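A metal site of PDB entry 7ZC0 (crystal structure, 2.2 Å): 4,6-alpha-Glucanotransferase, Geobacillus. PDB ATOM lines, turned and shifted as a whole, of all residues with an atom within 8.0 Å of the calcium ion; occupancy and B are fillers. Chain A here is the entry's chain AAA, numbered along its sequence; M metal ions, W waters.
The backbone carbonyl oxygen (O) of Asn 151 is in hydrogen-bond range of the backbone NH (N) of Glu 364 (3.2 Å). The backbone carbonyl oxygen of Asn 133 sits at hydrogen-bond distance from the backbone NH of Ile 371 (3.0 Å). A ring nitrogen (NE2) of His 405 sits at hydrogen-bond distance from the side-chain hydroxyl of Thr 404, at 3.3 Å. ND1 of His 405 lies within hydrogen-bond range of O of Tyr 363, 2.9 Å away. O of Asp 370 is in hydrogen-bond range of N of Asn 199, at 2.7 Å. The side-chain carboxylate (OE2) of Glu 364 lies close to the side-chain amide nitrogen (ND2) of Asn 199, 3.3 Å away. OE1 of Gln 134 sits at hydrogen-bond distance from ND2 of Asn 133, 2.7 Å away.
Merely in contact with the calcium ion: Phe 406 (3.99 Å). Of the 24 residues printed, 5 come within 4 Å of the calcium ion. The nearest printed residue that does not touch the calcium ion is Phe 365 (4.5 Å).
The calcium ion is bound by O of Glu 364. The calcium ion is bound by OE2 of Glu 364 (2.3 Å). O of His 405 is bound to the calcium ion (2.3 Å). The side-chain carboxylate (OD1) of Asp 370 is bound to the calcium ion (2.4 Å). OD1 of Asn 133 binds the calcium ion (2.4 Å). Water W1 is bound to the calcium ion, 2.6 Å away. The side-chain carboxylate (OD2) of Asp 370 binds the calcium ion, 2.6 Å away. The calcium ion has seven donor atoms within binding distance.
Water W1 lies within hydrogen-bond range of O of Asn 133, O of Ile 371 and ND2 of Asn 373.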
ATOM      1  N   PRO A 132      34.403  24.552  -4.060  1.00  0.00           N
ATOM      2  CA  PRO A 132      34.723  25.790  -4.789  1.00  0.00           C
ATOM      3  C   PRO A 132      33.517  26.626  -5.196  1.00  0.00           C
ATOM      4  O   PRO A 132      33.671  27.809  -5.468  1.00  0.00           O
ATOM      5  CB  PRO A 132      35.526  25.285  -6.015  1.00  0.00           C
ATOM      6  CG  PRO A 132      35.779  23.810  -5.739  1.00  0.00           C
ATOM      7  CD  PRO A 132      34.612  23.352  -4.882  1.00  0.00           C
ATOM      8  N   ASN A 133      32.310  26.012  -5.215  1.00  0.00           N
ATOM      9  CA  ASN A 133      31.135  26.575  -5.862  1.00  0.00           C
ATOM     10  C   ASN A 133      30.574  27.817  -5.179  1.00  0.00           C
ATOM     11  O   ASN A 133      30.160  28.738  -5.882  1.00  0.00           O
ATOM     12  CB  ASN A 133      29.994  25.557  -6.010  1.00  0.00           C
ATOM     13  CG  ASN A 133      28.864  26.187  -6.806  1.00  0.00           C
ATOM     14  OD1 ASN A 133      29.011  26.493  -7.996  1.00  0.00           O
ATOM     15  ND2 ASN A 133      27.762  26.448  -6.133  1.00  0.00           N
ATOM     16  N   GLN A 134      30.504  27.830  -3.827  1.00  0.00           N
ATOM     17  CA  GLN A 134      29.741  28.853  -3.124  1.00  0.00           C
ATOM     18  C   GLN A 134      30.272  29.101  -1.713  1.00  0.00           C
ATOM     19  O   GLN A 134      30.978  28.276  -1.136  1.00  0.00           O
ATOM     20  CB  GLN A 134      28.269  28.456  -2.965  1.00  0.00           C
ATOM     21  CG  GLN A 134      28.007  27.446  -1.852  1.00  0.00           C
ATOM     22  CD  GLN A 134      28.055  26.016  -2.343  1.00  0.00           C
ATOM     23  OE1 GLN A 134      27.963  25.752  -3.533  1.00  0.00           O
ATOM     24  NE2 GLN A 134      28.212  25.070  -1.421  1.00  0.00           N
ATOM     25  N   ASN A 151      18.334  28.106 -12.484  1.00  0.00           N
ATOM     26  CA  ASN A 151      19.611  27.478 -12.156  1.00  0.00           C
ATOM     27  C   ASN A 151      20.659  27.668 -13.254  1.00  0.00           C
ATOM     28  O   ASN A 151      21.878  27.630 -12.962  1.00  0.00           O
ATOM     29  CB  ASN A 151      19.404  26.007 -11.820  1.00  0.00           C
ATOM     30  CG  ASN A 151      18.683  25.307 -12.973  1.00  0.00           C
ATOM     31  OD1 ASN A 151      17.595  25.715 -13.350  1.00  0.00           O
ATOM     32  ND2 ASN A 151      19.334  24.354 -13.597  1.00  0.00           N
ATOM     33  N   ASN A 199      28.847  35.472  -9.030  1.00  0.00           N
ATOM     34  CA  ASN A 199      27.952  35.540 -10.158  1.00  0.00           C
ATOM     35  C   ASN A 199      26.561  35.976  -9.713  1.00  0.00           C
ATOM     36  O   ASN A 199      25.826  36.573 -10.483  1.00  0.00           O
ATOM     37  CB  ASN A 199      27.834  34.177 -10.857  1.00  0.00           C
ATOM     38  CG  ASN A 199      29.171  33.672 -11.356  1.00  0.00           C
ATOM     39  OD1 ASN A 199      30.014  34.441 -11.820  1.00  0.00           O
ATOM     40  ND2 ASN A 199      29.371  32.372 -11.294  1.00  0.00           N
ATOM     41  N   ASN A 354      30.886  35.425 -16.138  1.00  0.00           N
ATOM     42  CA  ASN A 354      30.722  34.379 -17.133  1.00  0.00           C
ATOM     43  C   ASN A 354      30.175  33.118 -16.476  1.00  0.00           C
ATOM     44  O   ASN A 354      30.869  32.504 -15.664  1.00  0.00           O
ATOM     45  CB  ASN A 354      32.048  33.979 -17.775  1.00  0.00           C
ATOM     46  CG  ASN A 354      31.880  33.087 -19.003  1.00  0.00           C
ATOM     47  OD1 ASN A 354      30.969  32.251 -19.099  1.00  0.00           O
ATOM     48  ND2 ASN A 354      32.780  33.254 -19.962  1.00  0.00           N
ATOM     49  N   ILE A 355      28.950  32.715 -16.864  1.00  0.00           N
ATOM     50  CA  ILE A 355      28.228  31.637 -16.218  1.00  0.00           C
ATOM     51  C   ILE A 355      28.060  30.434 -17.163  1.00  0.00           C
ATOM     52  O   ILE A 355      27.281  29.560 -16.809  1.00  0.00           O
ATOM     53  CB  ILE A 355      26.857  32.119 -15.675  1.00  0.00           C
ATOM     54  CG1 ILE A 355      25.918  32.623 -16.786  1.00  0.00           C
ATOM     55  CG2 ILE A 355      27.058  33.153 -14.575  1.00  0.00           C
ATOM     56  CD1 ILE A 355      24.454  32.773 -16.397  1.00  0.00           C
ATOM     57  N   THR A 358      30.922  25.981 -17.200  1.00  0.00           N
ATOM     58  CA  THR A 358      30.809  24.755 -16.408  1.00  0.00           C
ATOM     59  C   THR A 358      30.854  23.536 -17.327  1.00  0.00           C
ATOM     60  O   THR A 358      30.707  23.647 -18.535  1.00  0.00           O
ATOM     61  CB  THR A 358      29.457  24.686 -15.692  1.00  0.00           C
ATOM     62  OG1 THR A 358      28.455  24.566 -16.696  1.00  0.00           O
ATOM     63  CG2 THR A 358      29.155  25.884 -14.816  1.00  0.00           C
ATOM     64  N   ASN A 362      25.804  25.137 -18.658  1.00  0.00           N
ATOM     65  CA  ASN A 362      24.963  26.080 -17.933  1.00  0.00           C
ATOM     66  C   ASN A 362      24.935  25.593 -16.494  1.00  0.00           C
ATOM     67  O   ASN A 362      25.937  25.044 -16.055  1.00  0.00           O
ATOM     68  CB  ASN A 362      23.638  26.335 -18.649  1.00  0.00           C
ATOM     69  CG  ASN A 362      22.845  25.053 -18.855  1.00  0.00           C
ATOM     70  OD1 ASN A 362      23.243  23.980 -18.389  1.00  0.00           O
ATOM     71  ND2 ASN A 362      21.717  25.175 -19.532  1.00  0.00           N
ATOM     72  N   TYR A 363      23.825  25.753 -15.769  1.00  0.00           N
ATOM     73  CA  TYR A 363      23.716  25.203 -14.406  1.00  0.00           C
ATOM     74  C   TYR A 363      24.827  25.756 -13.499  1.00  0.00           C
ATOM     75  O   TYR A 363      25.489  25.059 -12.753  1.00  0.00           O
ATOM     76  CB  TYR A 363      23.704  23.661 -14.403  1.00  0.00           C
ATOM     77  CG  TYR A 363      22.711  23.038 -13.443  1.00  0.00           C
ATOM     78  CD1 TYR A 363      22.412  23.628 -12.226  1.00  0.00           C
ATOM     79  CD2 TYR A 363      22.076  21.830 -13.740  1.00  0.00           C
ATOM     80  CE1 TYR A 363      21.523  23.047 -11.322  1.00  0.00           C
ATOM     81  CE2 TYR A 363      21.166  21.228 -12.865  1.00  0.00           C
ATOM     82  CZ  TYR A 363      20.891  21.845 -11.643  1.00  0.00           C
ATOM     83  OH  TYR A 363      19.960  21.335 -10.780  1.00  0.00           O
ATOM     84  N   GLU A 364      25.014  27.061 -13.558  1.00  0.00           N
ATOM     85  CA  GLU A 364      26.034  27.703 -12.762  1.00  0.00           C
ATOM     86  C   GLU A 364      25.541  27.764 -11.310  1.00  0.00           C
ATOM     87  O   GLU A 364      26.346  27.707 -10.382  1.00  0.00           O
ATOM     88  CB  GLU A 364      26.283  29.083 -13.387  1.00  0.00           C
ATOM     89  CG  GLU A 364      27.334  29.923 -12.670  1.00  0.00           C
ATOM     90  CD  GLU A 364      28.743  29.381 -12.689  1.00  0.00           C
ATOM     91  OE1 GLU A 364      29.299  29.151 -13.828  1.00  0.00           O
ATOM     92  OE2 GLU A 364      29.280  29.124 -11.565  1.00  0.00           O
ATOM     93  N   PHE A 365      24.213  27.843 -11.123  1.00  0.00           N
ATOM     94  CA  PHE A 365      23.645  28.158  -9.816  1.00  0.00           C
ATOM     95  C   PHE A 365      23.066  26.944  -9.098  1.00  0.00           C
ATOM     96  O   PHE A 365      22.425  26.072  -9.702  1.00  0.00           O
ATOM     97  CB  PHE A 365      22.604  29.255  -9.968  1.00  0.00           C
ATOM     98  CG  PHE A 365      23.165  30.550 -10.511  1.00  0.00           C
ATOM     99  CD1 PHE A 365      23.846  31.425  -9.676  1.00  0.00           C
ATOM    100  CD2 PHE A 365      23.019  30.877 -11.850  1.00  0.00           C
ATOM    101  CE1 PHE A 365      24.364  32.623 -10.183  1.00  0.00           C
ATOM    102  CE2 PHE A 365      23.524  32.090 -12.334  1.00  0.00           C
ATOM    103  CZ  PHE A 365      24.225  32.943 -11.518  1.00  0.00           C
ATOM    104  N   LEU A 366      23.322  26.911  -7.780  1.00  0.00           N
ATOM    105  CA  LEU A 366      22.741  25.924  -6.899  1.00  0.00           C
ATOM    106  C   LEU A 366      22.098  26.627  -5.712  1.00  0.00           C
ATOM    107  O   LEU A 366      20.867  26.630  -5.591  1.00  0.00           O
ATOM    108  CB  LEU A 366      23.817  24.943  -6.416  1.00  0.00           C
ATOM    109  CG  LEU A 366      24.368  23.996  -7.471  1.00  0.00           C
ATOM    110  CD1 LEU A 366      25.583  23.252  -6.916  1.00  0.00           C
ATOM    111  CD2 LEU A 366      23.281  22.997  -7.894  1.00  0.00           C
ATOM    112  N   VAL A 367      22.955  27.167  -4.840  1.00  0.00           N
ATOM    113  CA  VAL A 367      22.539  27.720  -3.564  1.00  0.00           C
ATOM    114  C   VAL A 367      23.641  28.620  -2.991  1.00  0.00           C
ATOM    115  O   VAL A 367      24.826  28.363  -3.187  1.00  0.00           O
ATOM    116  CB  VAL A 367      22.093  26.620  -2.582  1.00  0.00           C
ATOM    117  CG1 VAL A 367      23.280  25.856  -1.989  1.00  0.00           C
ATOM    118  CG2 VAL A 367      21.217  27.182  -1.477  1.00  0.00           C
ATOM    119  N   LEU A 369      25.954  32.143  -2.104  1.00  0.00           N
ATOM    120  CA  LEU A 369      26.692  33.157  -2.864  1.00  0.00           C
ATOM    121  C   LEU A 369      27.561  32.414  -3.875  1.00  0.00           C
ATOM    122  O   LEU A 369      28.545  31.789  -3.484  1.00  0.00           O
ATOM    123  CB  LEU A 369      27.540  34.010  -1.904  1.00  0.00           C
ATOM    124  CG  LEU A 369      26.774  34.890  -0.912  1.00  0.00           C
ATOM    125  CD1 LEU A 369      27.712  35.440   0.160  1.00  0.00           C
ATOM    126  CD2 LEU A 369      26.058  36.045  -1.612  1.00  0.00           C
ATOM    127  N   ASP A 370      27.135  32.413  -5.140  1.00  0.00           N
ATOM    128  CA  ASP A 370      27.813  31.652  -6.170  1.00  0.00           C
ATOM    129  C   ASP A 370      29.095  32.363  -6.621  1.00  0.00           C
ATOM    130  O   ASP A 370      29.065  33.466  -7.166  1.00  0.00           O
ATOM    131  CB  ASP A 370      26.895  31.402  -7.363  1.00  0.00           C
ATOM    132  CG  ASP A 370      27.416  30.280  -8.271  1.00  0.00           C
ATOM    133  OD1 ASP A 370      27.465  29.130  -7.844  1.00  0.00           O
ATOM    134  OD2 ASP A 370      27.762  30.576  -9.401  1.00  0.00           O
ATOM    135  N   ILE A 371      30.221  31.669  -6.440  1.00  0.00           N
ATOM    136  CA  ILE A 371      31.558  32.180  -6.699  1.00  0.00           C
ATOM    137  C   ILE A 371      31.779  32.318  -8.207  1.00  0.00           C
ATOM    138  O   ILE A 371      31.500  31.385  -8.992  1.00  0.00           O
ATOM    139  CB  ILE A 371      32.573  31.265  -6.017  1.00  0.00           C
ATOM    140  CG1 ILE A 371      32.359  31.274  -4.501  1.00  0.00           C
ATOM    141  CG2 ILE A 371      33.992  31.693  -6.404  1.00  0.00           C
ATOM    142  CD1 ILE A 371      33.459  30.669  -3.637  1.00  0.00           C
ATOM    143  N   ASP A 372      32.274  33.506  -8.610  1.00  0.00           N
ATOM    144  CA  ASP A 372      32.649  33.745  -9.997  1.00  0.00           C
ATOM    145  C   ASP A 372      34.006  33.088 -10.289  1.00  0.00           C
ATOM    146  O   ASP A 372      35.047  33.756 -10.207  1.00  0.00           O
ATOM    147  CB  ASP A 372      32.670  35.248 -10.328  1.00  0.00           C
ATOM    148  CG  ASP A 372      32.847  35.505 -11.817  1.00  0.00           C
ATOM    149  OD1 ASP A 372      33.193  34.523 -12.576  1.00  0.00           O
ATOM    150  OD2 ASP A 372      32.604  36.684 -12.232  1.00  0.00           O
ATOM    151  N   ASN A 373      33.987  31.814 -10.709  1.00  0.00           N
ATOM    152  CA  ASN A 373      35.204  31.046 -10.848  1.00  0.00           C
ATOM    153  C   ASN A 373      35.865  31.348 -12.192  1.00  0.00           C
ATOM    154  O   ASN A 373      36.975  30.868 -12.465  1.00  0.00           O
ATOM    155  CB  ASN A 373      35.034  29.568 -10.478  1.00  0.00           C
ATOM    156  CG  ASN A 373      34.955  29.333  -8.987  1.00  0.00           C
ATOM    157  OD1 ASN A 373      35.975  29.333  -8.307  1.00  0.00           O
ATOM    158  ND2 ASN A 373      33.768  29.019  -8.457  1.00  0.00           N
ATOM    159  N   ALA A 402      30.109  19.688  -6.153  1.00  0.00           N
ATOM    160  CA  ALA A 402      29.395  20.411  -7.188  1.00  0.00           C
ATOM    161  C   ALA A 402      30.318  20.705  -8.366  1.00  0.00           C
ATOM    162  O   ALA A 402      30.167  21.755  -9.007  1.00  0.00           O
ATOM    163  CB  ALA A 402      28.777  21.666  -6.599  1.00  0.00           C
ATOM    164  N   THR A 404      30.390  20.213 -11.342  1.00  0.00           N
ATOM    165  CA  THR A 404      29.884  20.382 -12.704  1.00  0.00           C
ATOM    166  C   THR A 404      29.172  21.741 -12.835  1.00  0.00           C
ATOM    167  O   THR A 404      28.672  22.044 -13.919  1.00  0.00           O
ATOM    168  CB  THR A 404      28.967  19.242 -13.192  1.00  0.00           C
ATOM    169  OG1 THR A 404      27.854  19.129 -12.303  1.00  0.00           O
ATOM    170  CG2 THR A 404      29.679  17.910 -13.282  1.00  0.00           C
ATOM    171  N   HIS A 405      29.153  22.504 -11.726  1.00  0.00           N
ATOM    172  CA  HIS A 405      28.440  23.780 -11.572  1.00  0.00           C
ATOM    173  C   HIS A 405      29.316  25.046 -11.379  1.00  0.00           C
ATOM    174  O   HIS A 405      28.851  26.112 -10.935  1.00  0.00           O
ATOM    175  CB  HIS A 405      27.422  23.613 -10.436  1.00  0.00           C
ATOM    176  CG  HIS A 405      26.491  22.456 -10.609  1.00  0.00           C
ATOM    177  ND1 HIS A 405      25.346  22.527 -11.427  1.00  0.00           N
ATOM    178  CD2 HIS A 405      26.499  21.213 -10.056  1.00  0.00           C
ATOM    179  CE1 HIS A 405      24.722  21.361 -11.376  1.00  0.00           C
ATOM    180  NE2 HIS A 405      25.411  20.538 -10.552  1.00  0.00           N
ATOM    181  N   PHE A 406      30.585  24.995 -11.788  1.00  0.00           N
ATOM    182  CA  PHE A 406      31.417  26.192 -11.827  1.00  0.00           C
ATOM    183  C   PHE A 406      32.425  26.062 -12.962  1.00  0.00           C
ATOM    184  O   PHE A 406      32.553  24.992 -13.549  1.00  0.00           O
ATOM    185  CB  PHE A 406      32.069  26.475 -10.459  1.00  0.00           C
ATOM    186  CG  PHE A 406      32.808  25.331  -9.833  1.00  0.00           C
ATOM    187  CD1 PHE A 406      34.123  25.052 -10.188  1.00  0.00           C
ATOM    188  CD2 PHE A 406      32.201  24.519  -8.891  1.00  0.00           C
ATOM    189  CE1 PHE A 406      34.815  23.999  -9.587  1.00  0.00           C
ATOM    190  CE2 PHE A 406      32.886  23.452  -8.303  1.00  0.00           C
ATOM    191  CZ  PHE A 406      34.188  23.206  -8.657  1.00  0.00           C
ATOM    192  N   ASP A 407      33.108  27.181 -13.281  1.00  0.00           N
ATOM    193  CA  ASP A 407      34.134  27.234 -14.310  1.00  0.00           C
ATOM    194  C   ASP A 407      35.076  26.044 -14.175  1.00  0.00           C
ATOM    195  O   ASP A 407      35.732  25.873 -13.134  1.00  0.00           O
ATOM    196  CB  ASP A 407      34.871  28.577 -14.221  1.00  0.00           C
ATOM    197  CG  ASP A 407      35.679  28.907 -15.454  1.00  0.00           C
ATOM    198  OD1 ASP A 407      36.223  27.966 -16.032  1.00  0.00           O
ATOM    199  OD2 ASP A 407      35.738  30.141 -15.843  1.00  0.00           O
HETATM  200 CA    CA M   1      28.487  28.071  -9.708  1.00  0.00          CA
HETATM  201  O   HOH W   1      30.626  28.792  -8.424  1.00  0.00           O
